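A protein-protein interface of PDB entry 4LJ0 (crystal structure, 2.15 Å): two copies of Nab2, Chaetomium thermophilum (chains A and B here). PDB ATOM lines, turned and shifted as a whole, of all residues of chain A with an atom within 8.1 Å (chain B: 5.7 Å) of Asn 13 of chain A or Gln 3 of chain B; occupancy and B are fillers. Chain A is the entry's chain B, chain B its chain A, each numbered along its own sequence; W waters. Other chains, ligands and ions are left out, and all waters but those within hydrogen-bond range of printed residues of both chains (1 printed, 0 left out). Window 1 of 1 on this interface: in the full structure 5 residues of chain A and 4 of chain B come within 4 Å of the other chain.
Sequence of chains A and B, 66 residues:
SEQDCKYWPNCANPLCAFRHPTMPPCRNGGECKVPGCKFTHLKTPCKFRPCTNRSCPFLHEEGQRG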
ATOM      1  N   CYS A   5      36.826 -12.137 -22.018  1.00  0.00           N
ATOM      2  CA  CYS A   5      35.958 -11.520 -23.012  1.00  0.00           C
ATOM      3  C   CYS A   5      35.946 -10.008 -22.853  1.00  0.00           C
ATOM      4  O   CYS A   5      35.648  -9.485 -21.779  1.00  0.00           O
ATOM      5  CB  CYS A   5      34.530 -12.054 -22.904  1.00  0.00           C
ATOM      6  SG  CYS A   5      33.391 -11.289 -24.083  1.00  0.00           S
ATOM      7  N   TYR A   7      33.873  -8.062 -24.211  1.00  0.00           N
ATOM      8  CA  TYR A   7      32.512  -7.551 -24.370  1.00  0.00           C
ATOM      9  C   TYR A   7      31.613  -7.832 -23.168  1.00  0.00           C
ATOM     10  O   TYR A   7      30.639  -7.116 -22.937  1.00  0.00           O
ATOM     11  CB  TYR A   7      31.893  -8.139 -25.639  1.00  0.00           C
ATOM     12  CG  TYR A   7      32.686  -7.835 -26.892  1.00  0.00           C
ATOM     13  CD1 TYR A   7      32.552  -6.614 -27.544  1.00  0.00           C
ATOM     14  CD2 TYR A   7      33.569  -8.766 -27.422  1.00  0.00           C
ATOM     15  CE1 TYR A   7      33.276  -6.330 -28.685  1.00  0.00           C
ATOM     16  CE2 TYR A   7      34.298  -8.492 -28.563  1.00  0.00           C
ATOM     17  CZ  TYR A   7      34.147  -7.272 -29.191  1.00  0.00           C
ATOM     18  OH  TYR A   7      34.869  -6.995 -30.328  1.00  0.00           O
ATOM     19  N   TRP A   8      31.936  -8.874 -22.411  1.00  0.00           N
ATOM     20  CA  TRP A   8      31.186  -9.217 -21.207  1.00  0.00           C
ATOM     21  C   TRP A   8      31.153  -8.017 -20.256  1.00  0.00           C
ATOM     22  O   TRP A   8      32.154  -7.317 -20.115  1.00  0.00           O
ATOM     23  CB  TRP A   8      31.845 -10.420 -20.529  1.00  0.00           C
ATOM     24  CG  TRP A   8      31.069 -10.973 -19.383  1.00  0.00           C
ATOM     25  CD1 TRP A   8      30.124 -11.958 -19.430  1.00  0.00           C
ATOM     26  CD2 TRP A   8      31.160 -10.570 -18.013  1.00  0.00           C
ATOM     27  NE1 TRP A   8      29.627 -12.196 -18.173  1.00  0.00           N
ATOM     28  CE2 TRP A   8      30.248 -11.359 -17.285  1.00  0.00           C
ATOM     29  CE3 TRP A   8      31.933  -9.625 -17.330  1.00  0.00           C
ATOM     30  CZ2 TRP A   8      30.084 -11.228 -15.906  1.00  0.00           C
ATOM     31  CZ3 TRP A   8      31.769  -9.498 -15.962  1.00  0.00           C
ATOM     32  CH2 TRP A   8      30.851 -10.295 -15.264  1.00  0.00           C
ATOM     33  N   PRO A   9      30.012  -7.780 -19.577  1.00  0.00           N
ATOM     34  CA  PRO A   9      28.780  -8.570 -19.469  1.00  0.00           C
ATOM     35  C   PRO A   9      27.780  -8.269 -20.578  1.00  0.00           C
ATOM     36  O   PRO A   9      26.596  -8.581 -20.448  1.00  0.00           O
ATOM     37  CB  PRO A   9      28.224  -8.125 -18.120  1.00  0.00           C
ATOM     38  CG  PRO A   9      28.599  -6.682 -18.049  1.00  0.00           C
ATOM     39  CD  PRO A   9      29.912  -6.537 -18.791  1.00  0.00           C
ATOM     40  N   ASN A  10      28.264  -7.671 -21.658  1.00  0.00           N
ATOM     41  CA  ASN A  10      27.419  -7.315 -22.786  1.00  0.00           C
ATOM     42  C   ASN A  10      27.887  -8.036 -24.044  1.00  0.00           C
ATOM     43  O   ASN A  10      28.051  -7.432 -25.104  1.00  0.00           O
ATOM     44  CB  ASN A  10      27.428  -5.797 -22.973  1.00  0.00           C
ATOM     45  CG  ASN A  10      26.803  -5.068 -21.794  1.00  0.00           C
ATOM     46  OD1 ASN A  10      25.663  -5.340 -21.414  1.00  0.00           O
ATOM     47  ND2 ASN A  10      27.558  -4.157 -21.190  1.00  0.00           N
ATOM     48  N   CYS A  11      28.102  -9.341 -23.902  1.00  0.00           N
ATOM     49  CA  CYS A  11      28.563 -10.188 -24.992  1.00  0.00           C
ATOM     50  C   CYS A  11      27.374 -10.885 -25.642  1.00  0.00           C
ATOM     51  O   CYS A  11      26.708 -11.697 -25.007  1.00  0.00           O
ATOM     52  CB  CYS A  11      29.550 -11.228 -24.459  1.00  0.00           C
ATOM     53  SG  CYS A  11      30.219 -12.336 -25.715  1.00  0.00           S
ATOM     54  N   ALA A  12      27.113 -10.564 -26.907  1.00  0.00           N
ATOM     55  CA  ALA A  12      25.939 -11.082 -27.607  1.00  0.00           C
ATOM     56  C   ALA A  12      26.276 -12.282 -28.491  1.00  0.00           C
ATOM     57  O   ALA A  12      25.426 -12.762 -29.238  1.00  0.00           O
ATOM     58  CB  ALA A  12      25.304  -9.982 -28.443  1.00  0.00           C
ATOM     59  N   ASN A  13      27.517 -12.753 -28.412  1.00  0.00           N
ATOM     60  CA  ASN A  13      27.932 -13.936 -29.156  1.00  0.00           C
ATOM     61  C   ASN A  13      27.733 -15.173 -28.287  1.00  0.00           C
ATOM     62  O   ASN A  13      28.469 -15.373 -27.322  1.00  0.00           O
ATOM     63  CB  ASN A  13      29.399 -13.817 -29.576  1.00  0.00           C
ATOM     64  CG  ASN A  13      29.855 -14.967 -30.468  1.00  0.00           C
ATOM     65  OD1 ASN A  13      29.171 -15.981 -30.600  1.00  0.00           O
ATOM     66  ND2 ASN A  13      31.023 -14.811 -31.074  1.00  0.00           N
ATOM     67  N   PRO A  14      26.737 -16.012 -28.619  1.00  0.00           N
ATOM     68  CA  PRO A  14      26.512 -17.204 -27.795  1.00  0.00           C
ATOM     69  C   PRO A  14      27.663 -18.204 -27.895  1.00  0.00           C
ATOM     70  O   PRO A  14      27.832 -19.035 -27.004  1.00  0.00           O
ATOM     71  CB  PRO A  14      25.234 -17.802 -28.388  1.00  0.00           C
ATOM     72  CG  PRO A  14      25.222 -17.332 -29.799  1.00  0.00           C
ATOM     73  CD  PRO A  14      25.812 -15.958 -29.766  1.00  0.00           C
ATOM     74  N   LEU A  15      28.440 -18.114 -28.970  1.00  0.00           N
ATOM     75  CA  LEU A  15      29.568 -19.013 -29.189  1.00  0.00           C
ATOM     76  C   LEU A  15      30.883 -18.380 -28.750  1.00  0.00           C
ATOM     77  O   LEU A  15      31.954 -18.867 -29.112  1.00  0.00           O
ATOM     78  CB  LEU A  15      29.674 -19.377 -30.668  1.00  0.00           C
ATOM     79  CG  LEU A  15      28.448 -20.007 -31.323  1.00  0.00           C
ATOM     80  CD1 LEU A  15      28.726 -20.241 -32.799  1.00  0.00           C
ATOM     81  CD2 LEU A  15      28.067 -21.306 -30.628  1.00  0.00           C
ATOM     82  N   CYS A  16      30.805 -17.295 -27.986  1.00  0.00           N
ATOM     83  CA  CYS A  16      32.000 -16.568 -27.573  1.00  0.00           C
ATOM     84  C   CYS A  16      33.004 -17.487 -26.889  1.00  0.00           C
ATOM     85  O   CYS A  16      32.668 -18.201 -25.943  1.00  0.00           O
ATOM     86  CB  CYS A  16      31.640 -15.411 -26.645  1.00  0.00           C
ATOM     87  SG  CYS A  16      33.080 -14.550 -25.989  1.00  0.00           S
ATOM     88  N   ALA A  17      34.239 -17.463 -27.379  1.00  0.00           N
ATOM     89  CA  ALA A  17      35.285 -18.353 -26.890  1.00  0.00           C
ATOM     90  C   ALA A  17      36.049 -17.740 -25.719  1.00  0.00           C
ATOM     91  O   ALA A  17      36.604 -18.461 -24.890  1.00  0.00           O
ATOM     92  CB  ALA A  17      36.243 -18.701 -28.018  1.00  0.00           C
ATOM     93  N   PHE A  18      36.080 -16.412 -25.658  1.00  0.00           N
ATOM     94  CA  PHE A  18      36.752 -15.712 -24.569  1.00  0.00           C
ATOM     95  C   PHE A  18      36.074 -16.099 -23.257  1.00  0.00           C
ATOM     96  O   PHE A  18      34.893 -16.446 -23.252  1.00  0.00           O
ATOM     97  CB  PHE A  18      36.676 -14.195 -24.766  1.00  0.00           C
ATOM     98  CG  PHE A  18      37.141 -13.716 -26.122  1.00  0.00           C
ATOM     99  CD1 PHE A  18      37.953 -14.502 -26.926  1.00  0.00           C
ATOM    100  CD2 PHE A  18      36.764 -12.463 -26.586  1.00  0.00           C
ATOM    101  CE1 PHE A  18      38.372 -14.049 -28.166  1.00  0.00           C
ATOM    102  CE2 PHE A  18      37.181 -12.006 -27.821  1.00  0.00           C
ATOM    103  CZ  PHE A  18      37.986 -12.800 -28.613  1.00  0.00           C
ATOM    104  N   HIS A  20      34.167 -15.813 -19.763  1.00  0.00           N
ATOM    105  CA  HIS A  20      33.232 -14.934 -19.072  1.00  0.00           C
ATOM    106  C   HIS A  20      33.277 -15.262 -17.585  1.00  0.00           C
ATOM    107  O   HIS A  20      33.146 -16.427 -17.215  1.00  0.00           O
ATOM    108  CB  HIS A  20      31.812 -15.155 -19.586  1.00  0.00           C
ATOM    109  CG  HIS A  20      31.672 -15.009 -21.068  1.00  0.00           C
ATOM    110  ND1 HIS A  20      31.735 -16.083 -21.930  1.00  0.00           N
ATOM    111  CD2 HIS A  20      31.473 -13.917 -21.842  1.00  0.00           C
ATOM    112  CE1 HIS A  20      31.580 -15.659 -23.169  1.00  0.00           C
ATOM    113  NE2 HIS A  20      31.419 -14.348 -23.145  1.00  0.00           N
ATOM    114  N   GLU B   2      29.717 -21.414 -23.988  1.00  0.00           N
ATOM    115  CA  GLU B   2      28.262 -21.316 -24.025  1.00  0.00           C
ATOM    116  C   GLU B   2      27.743 -20.394 -22.930  1.00  0.00           C
ATOM    117  O   GLU B   2      28.132 -20.512 -21.768  1.00  0.00           O
ATOM    118  CB  GLU B   2      27.629 -22.698 -23.866  1.00  0.00           C
ATOM    119  CG  GLU B   2      27.912 -23.648 -25.016  1.00  0.00           C
ATOM    120  CD  GLU B   2      27.293 -23.189 -26.321  1.00  0.00           C
ATOM    121  OE1 GLU B   2      26.365 -22.354 -26.284  1.00  0.00           O
ATOM    122  OE2 GLU B   2      27.738 -23.665 -27.387  1.00  0.00           O
ATOM    123  N   GLN B   3      26.864 -19.476 -23.314  1.00  0.00           N
ATOM    124  CA  GLN B   3      26.209 -18.585 -22.369  1.00  0.00           C
ATOM    125  C   GLN B   3      24.768 -19.032 -22.165  1.00  0.00           C
ATOM    126  O   GLN B   3      24.117 -19.489 -23.103  1.00  0.00           O
ATOM    127  CB  GLN B   3      26.238 -17.145 -22.886  1.00  0.00           C
ATOM    128  CG  GLN B   3      27.574 -16.449 -22.710  1.00  0.00           C
ATOM    129  CD  GLN B   3      27.598 -15.074 -23.345  1.00  0.00           C
ATOM    130  OE1 GLN B   3      28.026 -14.915 -24.488  1.00  0.00           O
ATOM    131  NE2 GLN B   3      27.137 -14.070 -22.605  1.00  0.00           N
ATOM    132  N   ASP B   4      24.278 -18.903 -20.936  1.00  0.00           N
ATOM    133  CA  ASP B   4      22.903 -19.264 -20.617  1.00  0.00           C
ATOM    134  C   ASP B   4      21.929 -18.270 -21.223  1.00  0.00           C
ATOM    135  O   ASP B   4      22.135 -17.061 -21.143  1.00  0.00           O
ATOM    136  CB  ASP B   4      22.688 -19.299 -19.102  1.00  0.00           C
ATOM    137  CG  ASP B   4      23.432 -20.433 -18.429  1.00  0.00           C
ATOM    138  OD1 ASP B   4      23.999 -21.286 -19.142  1.00  0.00           O
ATOM    139  OD2 ASP B   4      23.437 -20.472 -17.179  1.00  0.00           O
ATOM    140  N   CYS B   5      20.862 -18.784 -21.822  1.00  0.00           N
ATOM    141  CA  CYS B   5      19.767 -17.934 -22.258  1.00  0.00           C
ATOM    142  C   CYS B   5      19.181 -17.248 -21.026  1.00  0.00           C
ATOM    143  O   CYS B   5      18.843 -17.912 -20.049  1.00  0.00           O
ATOM    144  CB  CYS B   5      18.699 -18.763 -22.965  1.00  0.00           C
ATOM    145  SG  CYS B   5      17.301 -17.800 -23.571  1.00  0.00           S
ATOM    146  N   ALA B  17      20.273 -19.624 -29.821  1.00  0.00           N
ATOM    147  CA  ALA B  17      21.551 -20.326 -29.827  1.00  0.00           C
ATOM    148  C   ALA B  17      22.197 -20.338 -28.446  1.00  0.00           C
ATOM    149  O   ALA B  17      23.232 -20.969 -28.244  1.00  0.00           O
ATOM    150  CB  ALA B  17      22.485 -19.691 -30.832  1.00  0.00           C
ATOM    151  N   PHE B  18      21.595 -19.629 -27.499  1.00  0.00           N
ATOM    152  CA  PHE B  18      22.102 -19.620 -26.136  1.00  0.00           C
ATOM    153  C   PHE B  18      21.675 -20.905 -25.433  1.00  0.00           C
ATOM    154  O   PHE B  18      20.744 -21.583 -25.867  1.00  0.00           O
ATOM    155  CB  PHE B  18      21.613 -18.376 -25.387  1.00  0.00           C
ATOM    156  CG  PHE B  18      22.245 -17.096 -25.874  1.00  0.00           C
ATOM    157  CD1 PHE B  18      21.820 -16.504 -27.052  1.00  0.00           C
ATOM    158  CD2 PHE B  18      23.265 -16.492 -25.158  1.00  0.00           C
ATOM    159  CE1 PHE B  18      22.399 -15.333 -27.507  1.00  0.00           C
ATOM    160  CE2 PHE B  18      23.849 -15.320 -25.605  1.00  0.00           C
ATOM    161  CZ  PHE B  18      23.415 -14.740 -26.784  1.00  0.00           C
ATOM    162  N   ARG B  19      22.365 -21.236 -24.350  1.00  0.00           N
ATOM    163  CA  ARG B  19      22.164 -22.509 -23.669  1.00  0.00           C
ATOM    164  C   ARG B  19      20.816 -22.575 -22.956  1.00  0.00           C
ATOM    165  O   ARG B  19      20.500 -21.719 -22.129  1.00  0.00           O
ATOM    166  CB  ARG B  19      23.292 -22.730 -22.662  1.00  0.00           C
ATOM    167  CG  ARG B  19      23.489 -24.171 -22.237  1.00  0.00           C
ATOM    168  CD  ARG B  19      24.532 -24.255 -21.137  1.00  0.00           C
ATOM    169  NE  ARG B  19      25.091 -25.596 -20.998  1.00  0.00           N
ATOM    170  CZ  ARG B  19      26.038 -25.921 -20.122  1.00  0.00           C
ATOM    171  NH1 ARG B  19      26.533 -25.003 -19.302  1.00  0.00           N
ATOM    172  NH2 ARG B  19      26.490 -27.167 -20.065  1.00  0.00           N
HETATM  173  O   HOH W   1      27.647 -11.262 -21.482  1.00  0.00           O
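O of Ala 12 of chain A touches CZ of Phe 18 of chain B (3.7 Å). Pro 14 of chain A touches Glu 2 of chain B. N of Gln 3 of chain B touches O of Pro 14 of chain A (3.8 Å). O of Ala 17 of chain B touches CB of Pro 14 of chain A (3.7 Å). CB of Pro 14 of chain A touches CE1 of Phe 18 of chain B, 3.9 Å away. His 20 of chain A touches Gln 3 of chain B (NE2 to OE1, 3.7 Å).
The side-chain amide nitrogen (NE2) of Gln 3 of chain B is in hydrogen-bond range of the backbone carbonyl oxygen (O) of Cys 11 of chain A (3.4 Å). O of Asn 13 of chain A sits close to OE1 of Gln 3 of chain B.
Asn 13 of chain A touches just one residue of chain B: Gln 3 (2.9 Å). Of the printed residues of chain A, Gln 3 of chain B touches Cys 11 (3.4 Å), Asn 13 (2.9 Å), Pro 14 (3.8 Å) and His 20 (3.7 Å). Printed residues of chain A within 4 Å of Phe 18 of chain B: Ala 12 (3.7 Å) and Pro 14 (3.9 Å). Of the printed residues of chain B, Ala 12 of chain A touches Phe 18. Of the printed residues of chain A, Glu 2 of chain B touches Pro 14. Of the printed residues of chain B, Cys 11 of chain A touches Gln 3. Asn 10 of chain A touches none of the printed residues of chain B. The nearest residue of chain B that does not touch Asn 13 of chain A is Phe 18 of chain B (4.6 Å). The nearest residue of chain A that does not touch Gln 3 of chain B is Cys 16 of chain A (4.2 Å).
Positions printed for both chains: 5, 17 and 18. Of the 8 pairs that touch across the chains among the printed residues, none has its exchanged pair printed and touching as well.
Of the 14 printed residues of chain A, 5 touch a printed residue of chain B. Printed residues of chain A that touch a printed residue of chain B: Cys 11, Ala 12, Asn 13, Pro 14 and His 20. Hydrophobic or aromatic side chains of chain A within 4 Å of the printed part of chain B: Pro 14 and His 20. Of the 7 printed residues of chain B, 4 touch a printed residue of chain A. Among the printed residues, no Asp or Glu carboxylate lies within 4 Å of a Lys or Arg side-chain nitrogen of the other chain.
O of Gln 3 of chain B is in hydrogen-bond range of N of Arg 19 of chain B, 2.8 Å away. The side-chain amide oxygen of Asn 13 of chain A is in hydrogen-bond range of the backbone NH of Leu 15 of chain A (2.8 Å). N of Cys 16 of chain A lies within hydrogen-bond range of OD1 of Asn 13 of chain A (3.4 Å). O of Phe 18 of chain A lies close to ND1 of His 20 of chain A (3.4 Å).
Water W1 lies within hydrogen-bond range of O of Pro 9 of chain A (3.1 Å), NE2 of Gln 3 of chain B (3.1 Å) and N of Cys 11 of chain A (3.1 Å).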
